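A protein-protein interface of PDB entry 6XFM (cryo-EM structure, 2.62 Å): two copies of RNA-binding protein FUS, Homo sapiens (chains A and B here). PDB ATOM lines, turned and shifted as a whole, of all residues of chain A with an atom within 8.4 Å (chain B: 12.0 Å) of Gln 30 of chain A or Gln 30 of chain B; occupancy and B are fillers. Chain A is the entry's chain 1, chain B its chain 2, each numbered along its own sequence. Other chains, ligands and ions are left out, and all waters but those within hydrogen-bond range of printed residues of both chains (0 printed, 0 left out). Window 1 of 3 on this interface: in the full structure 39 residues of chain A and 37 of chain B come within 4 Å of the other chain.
Gln 8 of chain A touches three residues of chain B.
Of the printed residues of chain B, Ser 9 of chain A touches Ser 9.
Of chain B, only Ser 9 (3.0 Å), Ser 10 (3.3 Å) and Ser 11 (3.2 Å) come within 4 Å of Ser 10 of chain A.
Of the printed residues of chain B, Ser 11 of chain A touches Ser 11 (3.4 Å).
Gly 28 of chain A touches just these residues of chain B: Gly 28 (3.6 Å) and Gln 29 (2.9 Å).
Of chain B, only Gln 29 comes within 4 Å of Gln 29 of chain A.
Of chain B, only Gln 31 comes within 4 Å of Gln 31 of chain A.
Printed residues of chain A within 4 Å of Tyr 26 of chain B: Gly 27.
Gly 27 of chain B touches none of the printed residues of chain A.
Gln 30 of chain B touches just one residue of chain A: Gln 30 (3.1 Å).
Of the printed residues of chain A, Gln 31 of chain B touches Gln 30 (3.0 Å), Gln 31 (2.9 Å) and Ser 32 (2.9 Å).
Gly 34 of chain B touches none of the printed residues of chain A.
The nearest residue of chain B that does not touch Gln 30 of chain A is Gln 8 of chain B (4.05 Å).
The nearest residue of chain A that does not touch Gln 30 of chain B is Gly 28 of chain A (5.4 Å).
The backbone carbonyl oxygen of Gln 31 of chain A is in hydrogen-bond range of the side-chain amide nitrogen of Gln 8 of chain A, at 3.2 Å.
NE2 of Gln 30 of chain A is in hydrogen-bond range of OG of Ser 10 of chain A, at 2.8 Å.
The side-chain hydroxyl (OG) of Ser 32 of chain B sits at hydrogen-bond distance from the side-chain hydroxyl (OG) of Ser 6 of chain B.
The side-chain hydroxyl of Ser 6 of chain B lies within hydrogen-bond range of the backbone carbonyl oxygen of Tyr 33 of chain B, 3.2 Å away.
NE2 of Gln 8 of chain B sits at hydrogen-bond distance from O of Gln 31 of chain B (3.2 Å).
OG of Ser 10 of chain B sits at hydrogen-bond distance from NE2 of Gln 30 of chain B (2.8 Å).
The backbone carbonyl oxygen of Ser 7 of chain B is in hydrogen-bond range of the backbone NH of Gln 8 of chain A, 3.0 Å away.
The side-chain amide oxygen (OE1) of Gln 8 of chain A lies within hydrogen-bond range of the side-chain amide nitrogen (NE2) of Gln 8 of chain B (2.9 Å).
The backbone carbonyl oxygen of Gln 8 of chain A sits at hydrogen-bond distance from the backbone NH of Ser 9 of chain B (2.9 Å).
O of Ser 9 of chain B is in hydrogen-bond range of N of Ser 10 of chain A (3.0 Å).
The backbone carbonyl oxygen of Ser 10 of chain A lies within hydrogen-bond range of the backbone NH of Ser 11 of chain B (3.2 Å).
O of Ser 11 of chain B is in hydrogen-bond range of N of Tyr 12 of chain A, at 3.1 Å.
N of Gly 27 of chain A lies within hydrogen-bond range of O of Tyr 26 of chain B (3.1 Å).
The backbone carbonyl oxygen (O) of Gly 28 of chain A is in hydrogen-bond range of the backbone NH (N) of Gln 29 of chain B.
The side-chain amide nitrogen of Gln 29 of chain A sits at hydrogen-bond distance from the side-chain amide oxygen of Gln 29 of chain B (3.1 Å).
The backbone carbonyl oxygen (O) of Gln 29 of chain B is in hydrogen-bond range of the backbone NH (N) of Gln 30 of chain A (3.1 Å).
OE1 of Gln 30 of chain A sits at hydrogen-bond distance from NE2 of Gln 30 of chain B (3.1 Å).
N of Gln 31 of chain B lies within hydrogen-bond range of O of Gln 30 of chain A.
NE2 of Gln 31 of chain A lies within hydrogen-bond range of OE1 of Gln 31 of chain B, 2.9 Å away.
The backbone NH of Ser 32 of chain A is in hydrogen-bond range of the backbone carbonyl oxygen of Gln 31 of chain B (2.9 Å).
The backbone carbonyl oxygen (O) of Ser 32 of chain A is in hydrogen-bond range of the backbone NH (N) of Tyr 33 of chain B (2.8 Å).
Among the printed residues, pairs that only touch across the chains: Ser 9 of chain A with Ser 9 of chain B (3.4 Å), Ser 10 of chain A with Ser 10 of chain B (3.3 Å), Ser 11 of chain A with Ser 11 of chain B (3.4 Å), Tyr 12 of chain A with Tyr 12 of chain B (3.1 Å), Gly 27 of chain A with Gly 28 of chain B (3.7 Å), Gly 28 of chain A with Gly 28 of chain B (3.6 Å), Ser 32 of chain A with Ser 6 of chain B (3.6 Å), Ser 32 of chain A with Gln 8 of chain B (3.5 Å), Ser 32 of chain A with Ser 32 of chain B (3.7 Å) and Tyr 33 of chain A with Tyr 33 of chain B (3.4 Å).
Hydrophobic or aromatic side chains of chain B that line the printed part of chain A: Tyr 12 and Tyr 33.
Hydrophobic or aromatic side chains of chain A within 4 Å of the printed part of chain B: Tyr 12 and Tyr 33.
Among the printed residues, 25 pairs touch across the chains.
Ser 9 of chain B touches its own counterpart, Ser 9 of chain A.
Ser 10 of chain A touches Ser 9 of chain B, but with the chains exchanged Ser 9 of chain A does not touch Ser 10 of chain B (5.6 Å).
Ser 10 of chain A touches Ser 11 of chain B, but with the chains exchanged Ser 11 of chain A does not touch Ser 10 of chain B (5.5 Å).
Tyr 12 of chain A touches its own counterpart, Tyr 12 of chain B.
Of the 25 pairs that touch across the chains among the printed residues, 11 have their exchanged pair printed and touching as well.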
ATOM      1  N   GLN A   8      26.633   8.714  -0.502  1.00  0.00           N
ATOM      2  CA  GLN A   8      26.388   7.619  -1.435  1.00  0.00           C
ATOM      3  C   GLN A   8      27.687   6.879  -1.737  1.00  0.00           C
ATOM      4  O   GLN A   8      28.723   7.503  -1.972  1.00  0.00           O
ATOM      5  CB  GLN A   8      25.799   8.162  -2.737  1.00  0.00           C
ATOM      6  CG  GLN A   8      24.386   8.681  -2.481  1.00  0.00           C
ATOM      7  CD  GLN A   8      23.859   9.391  -3.721  1.00  0.00           C
ATOM      8  OE1 GLN A   8      24.633   9.967  -4.485  1.00  0.00           O
ATOM      9  NE2 GLN A   8      22.579   9.380  -3.972  1.00  0.00           N
ATOM     10  N   SER A   9      27.626   5.551  -1.736  1.00  0.00           N
ATOM     11  CA  SER A   9      28.807   4.744  -2.019  1.00  0.00           C
ATOM     12  C   SER A   9      28.486   3.665  -3.049  1.00  0.00           C
ATOM     13  O   SER A   9      27.475   2.971  -2.939  1.00  0.00           O
ATOM     14  CB  SER A   9      29.314   4.088  -0.733  1.00  0.00           C
ATOM     15  OG  SER A   9      29.670   5.099   0.200  1.00  0.00           O
ATOM     16  N   SER A  10      29.358   3.525  -4.041  1.00  0.00           N
ATOM     17  CA  SER A  10      29.171   2.518  -5.082  1.00  0.00           C
ATOM     18  C   SER A  10      30.499   1.833  -5.402  1.00  0.00           C
ATOM     19  O   SER A  10      31.550   2.480  -5.430  1.00  0.00           O
ATOM     20  CB  SER A  10      28.613   3.174  -6.347  1.00  0.00           C
ATOM     21  OG  SER A  10      27.343   3.745  -6.059  1.00  0.00           O
ATOM     22  N   SER A  11      30.463   0.527  -5.651  1.00  0.00           N
ATOM     23  CA  SER A  11      31.695  -0.189  -5.966  1.00  0.00           C
ATOM     24  C   SER A  11      31.444  -1.347  -6.928  1.00  0.00           C
ATOM     25  O   SER A  11      30.363  -1.933  -6.950  1.00  0.00           O
ATOM     26  CB  SER A  11      32.328  -0.725  -4.679  1.00  0.00           C
ATOM     27  OG  SER A  11      31.464  -1.695  -4.099  1.00  0.00           O
ATOM     28  N   TYR A  12      32.472  -1.674  -7.708  1.00  0.00           N
ATOM     29  CA  TYR A  12      32.398  -2.770  -8.670  1.00  0.00           C
ATOM     30  C   TYR A  12      33.607  -3.687  -8.497  1.00  0.00           C
ATOM     31  O   TYR A  12      34.719  -3.208  -8.258  1.00  0.00           O
ATOM     32  CB  TYR A  12      32.393  -2.212 -10.093  1.00  0.00           C
ATOM     33  CG  TYR A  12      31.180  -1.336 -10.296  1.00  0.00           C
ATOM     34  CD1 TYR A  12      31.234   0.022  -9.963  1.00  0.00           C
ATOM     35  CD2 TYR A  12      30.007  -1.879 -10.833  1.00  0.00           C
ATOM     36  CE1 TYR A  12      30.114   0.838 -10.166  1.00  0.00           C
ATOM     37  CE2 TYR A  12      28.887  -1.062 -11.034  1.00  0.00           C
ATOM     38  CZ  TYR A  12      28.941   0.296 -10.701  1.00  0.00           C
ATOM     39  OH  TYR A  12      27.838   1.100 -10.902  1.00  0.00           O
ATOM     40  N   GLY A  27      27.890   4.309 -17.321  1.00  0.00           N
ATOM     41  CA  GLY A  27      27.624   4.753 -15.954  1.00  0.00           C
ATOM     42  C   GLY A  27      26.199   5.299 -15.831  1.00  0.00           C
ATOM     43  O   GLY A  27      25.579   5.654 -16.831  1.00  0.00           O
ATOM     44  N   GLY A  28      25.680   5.356 -14.606  1.00  0.00           N
ATOM     45  CA  GLY A  28      24.320   5.853 -14.385  1.00  0.00           C
ATOM     46  C   GLY A  28      24.317   7.266 -13.802  1.00  0.00           C
ATOM     47  O   GLY A  28      25.272   8.022 -13.982  1.00  0.00           O
ATOM     48  N   GLN A  29      23.222   7.616 -13.118  1.00  0.00           N
ATOM     49  CA  GLN A  29      23.076   8.948 -12.524  1.00  0.00           C
ATOM     50  C   GLN A  29      22.903   8.879 -11.004  1.00  0.00           C
ATOM     51  O   GLN A  29      22.132   8.064 -10.498  1.00  0.00           O
ATOM     52  CB  GLN A  29      21.838   9.634 -13.109  1.00  0.00           C
ATOM     53  CG  GLN A  29      22.074   9.977 -14.574  1.00  0.00           C
ATOM     54  CD  GLN A  29      20.766  10.437 -15.205  1.00  0.00           C
ATOM     55  OE1 GLN A  29      19.691  10.002 -14.792  1.00  0.00           O
ATOM     56  NE2 GLN A  29      20.791  11.297 -16.183  1.00  0.00           N
ATOM     57  N   GLN A  30      23.595   9.772 -10.293  1.00  0.00           N
ATOM     58  CA  GLN A  30      23.485   9.845  -8.836  1.00  0.00           C
ATOM     59  C   GLN A  30      23.341  11.304  -8.394  1.00  0.00           C
ATOM     60  O   GLN A  30      24.061  12.178  -8.874  1.00  0.00           O
ATOM     61  CB  GLN A  30      24.725   9.246  -8.161  1.00  0.00           C
ATOM     62  CG  GLN A  30      24.754   7.727  -8.359  1.00  0.00           C
ATOM     63  CD  GLN A  30      26.069   7.160  -7.828  1.00  0.00           C
ATOM     64  OE1 GLN A  30      27.084   7.854  -7.814  1.00  0.00           O
ATOM     65  NE2 GLN A  30      26.110   5.930  -7.386  1.00  0.00           N
ATOM     66  N   GLN A  31      22.424  11.559  -7.463  1.00  0.00           N
ATOM     67  CA  GLN A  31      22.214  12.914  -6.950  1.00  0.00           C
ATOM     68  C   GLN A  31      22.120  12.908  -5.431  1.00  0.00           C
ATOM     69  O   GLN A  31      21.278  12.222  -4.850  1.00  0.00           O
ATOM     70  CB  GLN A  31      20.950  13.537  -7.552  1.00  0.00           C
ATOM     71  CG  GLN A  31      21.290  14.188  -8.894  1.00  0.00           C
ATOM     72  CD  GLN A  31      20.051  14.856  -9.480  1.00  0.00           C
ATOM     73  OE1 GLN A  31      18.930  14.427  -9.216  1.00  0.00           O
ATOM     74  NE2 GLN A  31      20.189  15.888 -10.266  1.00  0.00           N
ATOM     75  N   SER A  32      22.997  13.674  -4.795  1.00  0.00           N
ATOM     76  CA  SER A  32      23.014  13.748  -3.344  1.00  0.00           C
ATOM     77  C   SER A  32      22.746  15.168  -2.873  1.00  0.00           C
ATOM     78  O   SER A  32      23.429  16.106  -3.288  1.00  0.00           O
ATOM     79  CB  SER A  32      24.372  13.290  -2.817  1.00  0.00           C
ATOM     80  OG  SER A  32      24.419  13.480  -1.411  1.00  0.00           O
ATOM     81  N   TYR A  33      21.759  15.313  -1.997  1.00  0.00           N
ATOM     82  CA  TYR A  33      21.414  16.622  -1.459  1.00  0.00           C
ATOM     83  C   TYR A  33      21.614  16.656   0.055  1.00  0.00           C
ATOM     84  O   TYR A  33      21.014  15.869   0.788  1.00  0.00           O
ATOM     85  CB  TYR A  33      19.950  16.956  -1.750  1.00  0.00           C
ATOM     86  CG  TYR A  33      19.694  17.093  -3.237  1.00  0.00           C
ATOM     87  CD1 TYR A  33      19.828  18.341  -3.856  1.00  0.00           C
ATOM     88  CD2 TYR A  33      19.284  15.982  -3.985  1.00  0.00           C
ATOM     89  CE1 TYR A  33      19.549  18.480  -5.222  1.00  0.00           C
ATOM     90  CE2 TYR A  33      19.011  16.119  -5.352  1.00  0.00           C
ATOM     91  CZ  TYR A  33      19.140  17.368  -5.971  1.00  0.00           C
ATOM     92  OH  TYR A  33      18.868  17.501  -7.318  1.00  0.00           O
ATOM     93  N   SER B   6      27.555  16.778   2.073  1.00  0.00           N
ATOM     94  CA  SER B   6      27.286  15.644   1.201  1.00  0.00           C
ATOM     95  C   SER B   6      28.598  15.029   0.724  1.00  0.00           C
ATOM     96  O   SER B   6      29.609  15.723   0.585  1.00  0.00           O
ATOM     97  CB  SER B   6      26.457  16.093  -0.001  1.00  0.00           C
ATOM     98  OG  SER B   6      27.197  17.050  -0.746  1.00  0.00           O
ATOM     99  N   SER B   7      28.585  13.724   0.475  1.00  0.00           N
ATOM    100  CA  SER B   7      29.795  13.046   0.021  1.00  0.00           C
ATOM    101  C   SER B   7      29.459  11.845  -0.858  1.00  0.00           C
ATOM    102  O   SER B   7      28.512  11.109  -0.587  1.00  0.00           O
ATOM    103  CB  SER B   7      30.614  12.581   1.226  1.00  0.00           C
ATOM    104  OG  SER B   7      31.787  11.919   0.769  1.00  0.00           O
ATOM    105  N   GLN B   8      30.255  11.646  -1.905  1.00  0.00           N
ATOM    106  CA  GLN B   8      30.043  10.523  -2.811  1.00  0.00           C
ATOM    107  C   GLN B   8      31.355   9.788  -3.057  1.00  0.00           C
ATOM    108  O   GLN B   8      32.391  10.412  -3.282  1.00  0.00           O
ATOM    109  CB  GLN B   8      29.484  11.024  -4.144  1.00  0.00           C
ATOM    110  CG  GLN B   8      28.059  11.537  -3.938  1.00  0.00           C
ATOM    111  CD  GLN B   8      27.560  12.207  -5.212  1.00  0.00           C
ATOM    112  OE1 GLN B   8      28.350  12.768  -5.972  1.00  0.00           O
ATOM    113  NE2 GLN B   8      26.288  12.180  -5.496  1.00  0.00           N
ATOM    114  N   SER B   9      31.305   8.458  -3.020  1.00  0.00           N
ATOM    115  CA  SER B   9      32.501   7.657  -3.249  1.00  0.00           C
ATOM    116  C   SER B   9      32.218   6.548  -4.258  1.00  0.00           C
ATOM    117  O   SER B   9      31.209   5.849  -4.159  1.00  0.00           O
ATOM    118  CB  SER B   9      32.978   7.040  -1.933  1.00  0.00           C
ATOM    119  OG  SER B   9      33.302   8.079  -1.018  1.00  0.00           O
ATOM    120  N   SER B  10      33.122   6.385  -5.219  1.00  0.00           N
ATOM    121  CA  SER B  10      32.970   5.348  -6.236  1.00  0.00           C
ATOM    122  C   SER B  10      34.313   4.668  -6.503  1.00  0.00           C
ATOM    123  O   SER B  10      35.353   5.326  -6.528  1.00  0.00           O
ATOM    124  CB  SER B  10      32.441   5.962  -7.532  1.00  0.00           C
ATOM    125  OG  SER B  10      31.161   6.532  -7.292  1.00  0.00           O
ATOM    126  N   SER B  11      34.295   3.353  -6.706  1.00  0.00           N
ATOM    127  CA  SER B  11      35.541   2.639  -6.971  1.00  0.00           C
ATOM    128  C   SER B  11      35.326   1.451  -7.906  1.00  0.00           C
ATOM    129  O   SER B  11      34.253   0.850  -7.934  1.00  0.00           O
ATOM    130  CB  SER B  11      36.144   2.147  -5.654  1.00  0.00           C
ATOM    131  OG  SER B  11      35.274   1.187  -5.070  1.00  0.00           O
ATOM    132  N   TYR B  12      36.378   1.116  -8.652  1.00  0.00           N
ATOM    133  CA  TYR B  12      36.340  -0.009  -9.585  1.00  0.00           C
ATOM    134  C   TYR B  12      37.554  -0.909  -9.353  1.00  0.00           C
ATOM    135  O   TYR B  12      38.653  -0.414  -9.105  1.00  0.00           O
ATOM    136  CB  TYR B  12      36.369   0.509 -11.023  1.00  0.00           C
ATOM    137  CG  TYR B  12      35.155   1.369 -11.287  1.00  0.00           C
ATOM    138  CD1 TYR B  12      35.189   2.736 -10.989  1.00  0.00           C
ATOM    139  CD2 TYR B  12      34.004   0.802 -11.842  1.00  0.00           C
ATOM    140  CE1 TYR B  12      34.069   3.536 -11.246  1.00  0.00           C
ATOM    141  CE2 TYR B  12      32.883   1.602 -12.098  1.00  0.00           C
ATOM    142  CZ  TYR B  12      32.916   2.968 -11.800  1.00  0.00           C
ATOM    143  OH  TYR B  12      31.812   3.756 -12.052  1.00  0.00           O
ATOM    144  N   TYR B  26      32.290   3.835 -20.462  1.00  0.00           N
ATOM    145  CA  TYR B  26      31.859   5.231 -20.427  1.00  0.00           C
ATOM    146  C   TYR B  26      31.488   5.634 -18.998  1.00  0.00           C
ATOM    147  O   TYR B  26      30.739   4.925 -18.324  1.00  0.00           O
ATOM    148  CB  TYR B  26      30.631   5.429 -21.320  1.00  0.00           C
ATOM    149  CG  TYR B  26      30.961   5.091 -22.750  1.00  0.00           C
ATOM    150  CD1 TYR B  26      30.771   3.788 -23.221  1.00  0.00           C
ATOM    151  CD2 TYR B  26      31.424   6.087 -23.614  1.00  0.00           C
ATOM    152  CE1 TYR B  26      31.041   3.480 -24.560  1.00  0.00           C
ATOM    153  CE2 TYR B  26      31.702   5.781 -24.949  1.00  0.00           C
ATOM    154  CZ  TYR B  26      31.508   4.479 -25.425  1.00  0.00           C
ATOM    155  OH  TYR B  26      31.762   4.186 -26.749  1.00  0.00           O
ATOM    156  N   GLY B  27      31.998   6.779 -18.549  1.00  0.00           N
ATOM    157  CA  GLY B  27      31.692   7.259 -17.201  1.00  0.00           C
ATOM    158  C   GLY B  27      30.260   7.793 -17.133  1.00  0.00           C
ATOM    159  O   GLY B  27      29.663   8.111 -18.161  1.00  0.00           O
ATOM    160  N   GLY B  28      29.707   7.883 -15.926  1.00  0.00           N
ATOM    161  CA  GLY B  28      28.337   8.372 -15.757  1.00  0.00           C
ATOM    162  C   GLY B  28      28.305   9.802 -15.214  1.00  0.00           C
ATOM    163  O   GLY B  28      29.256  10.563 -15.394  1.00  0.00           O
ATOM    164  N   GLN B  29      27.190  10.159 -14.569  1.00  0.00           N
ATOM    165  CA  GLN B  29      27.016  11.506 -14.016  1.00  0.00           C
ATOM    166  C   GLN B  29      26.801  11.481 -12.501  1.00  0.00           C
ATOM    167  O   GLN B  29      26.020  10.679 -11.992  1.00  0.00           O
ATOM    168  CB  GLN B  29      25.788  12.162 -14.653  1.00  0.00           C
ATOM    169  CG  GLN B  29      26.060  12.467 -16.121  1.00  0.00           C
ATOM    170  CD  GLN B  29      24.763  12.895 -16.798  1.00  0.00           C
ATOM    171  OE1 GLN B  29      23.684  12.459 -16.402  1.00  0.00           O
ATOM    172  NE2 GLN B  29      24.806  13.728 -17.799  1.00  0.00           N
ATOM    173  N   GLN B  30      27.471  12.398 -11.797  1.00  0.00           N
ATOM    174  CA  GLN B  30      27.322  12.512 -10.348  1.00  0.00           C
ATOM    175  C   GLN B  30      27.152  13.981  -9.950  1.00  0.00           C
ATOM    176  O   GLN B  30      27.879  14.847 -10.433  1.00  0.00           O
ATOM    177  CB  GLN B  30      28.547  11.944  -9.624  1.00  0.00           C
ATOM    178  CG  GLN B  30      28.595  10.420  -9.777  1.00  0.00           C
ATOM    179  CD  GLN B  30      29.901   9.882  -9.196  1.00  0.00           C
ATOM    180  OE1 GLN B  30      30.909  10.585  -9.179  1.00  0.00           O
ATOM    181  NE2 GLN B  30      29.940   8.668  -8.716  1.00  0.00           N
ATOM    182  N   GLN B  31      26.208  14.254  -9.054  1.00  0.00           N
ATOM    183  CA  GLN B  31      25.973  15.621  -8.584  1.00  0.00           C
ATOM    184  C   GLN B  31      25.838  15.655  -7.070  1.00  0.00           C
ATOM    185  O   GLN B  31      24.987  14.977  -6.493  1.00  0.00           O
ATOM    186  CB  GLN B  31      24.722  16.217  -9.236  1.00  0.00           C
ATOM    187  CG  GLN B  31      25.093  16.830 -10.588  1.00  0.00           C
ATOM    188  CD  GLN B  31      23.864  17.467 -11.226  1.00  0.00           C
ATOM    189  OE1 GLN B  31      22.740  17.034 -10.981  1.00  0.00           O
ATOM    190  NE2 GLN B  31      24.012  18.477 -12.040  1.00  0.00           N
ATOM    191  N   SER B  32      26.690  16.447  -6.431  1.00  0.00           N
ATOM    192  CA  SER B  32      26.668  16.562  -4.983  1.00  0.00           C
ATOM    193  C   SER B  32      26.374  17.993  -4.558  1.00  0.00           C
ATOM    194  O   SER B  32      27.059  18.926  -4.980  1.00  0.00           O
ATOM    195  CB  SER B  32      28.017  16.134  -4.408  1.00  0.00           C
ATOM    196  OG  SER B  32      28.023  16.364  -3.006  1.00  0.00           O
ATOM    197  N   TYR B  33      25.362  18.153  -3.715  1.00  0.00           N
ATOM    198  CA  TYR B  33      24.992  19.474  -3.224  1.00  0.00           C
ATOM    199  C   TYR B  33      25.150  19.554  -1.708  1.00  0.00           C
ATOM    200  O   TYR B  33      24.532  18.787  -0.971  1.00  0.00           O
ATOM    201  CB  TYR B  33      23.533  19.784  -3.565  1.00  0.00           C
ATOM    202  CG  TYR B  33      23.316  19.877  -5.060  1.00  0.00           C
ATOM    203  CD1 TYR B  33      23.455  21.108  -5.711  1.00  0.00           C
ATOM    204  CD2 TYR B  33      22.938  18.740  -5.787  1.00  0.00           C
ATOM    205  CE1 TYR B  33      23.212  21.205  -7.087  1.00  0.00           C
ATOM    206  CE2 TYR B  33      22.703  18.836  -7.164  1.00  0.00           C
ATOM    207  CZ  TYR B  33      22.837  20.068  -7.815  1.00  0.00           C
ATOM    208  OH  TYR B  33      22.599  20.160  -9.171  1.00  0.00           O
ATOM    209  N   GLY B  34      25.948  20.509  -1.253  1.00  0.00           N
ATOM    210  CA  GLY B  34      26.152  20.718   0.178  1.00  0.00           C
ATOM    211  C   GLY B  34      26.062  22.207   0.479  1.00  0.00           C
ATOM    212  O   GLY B  34      26.966  22.964   0.138  1.00  0.00           O
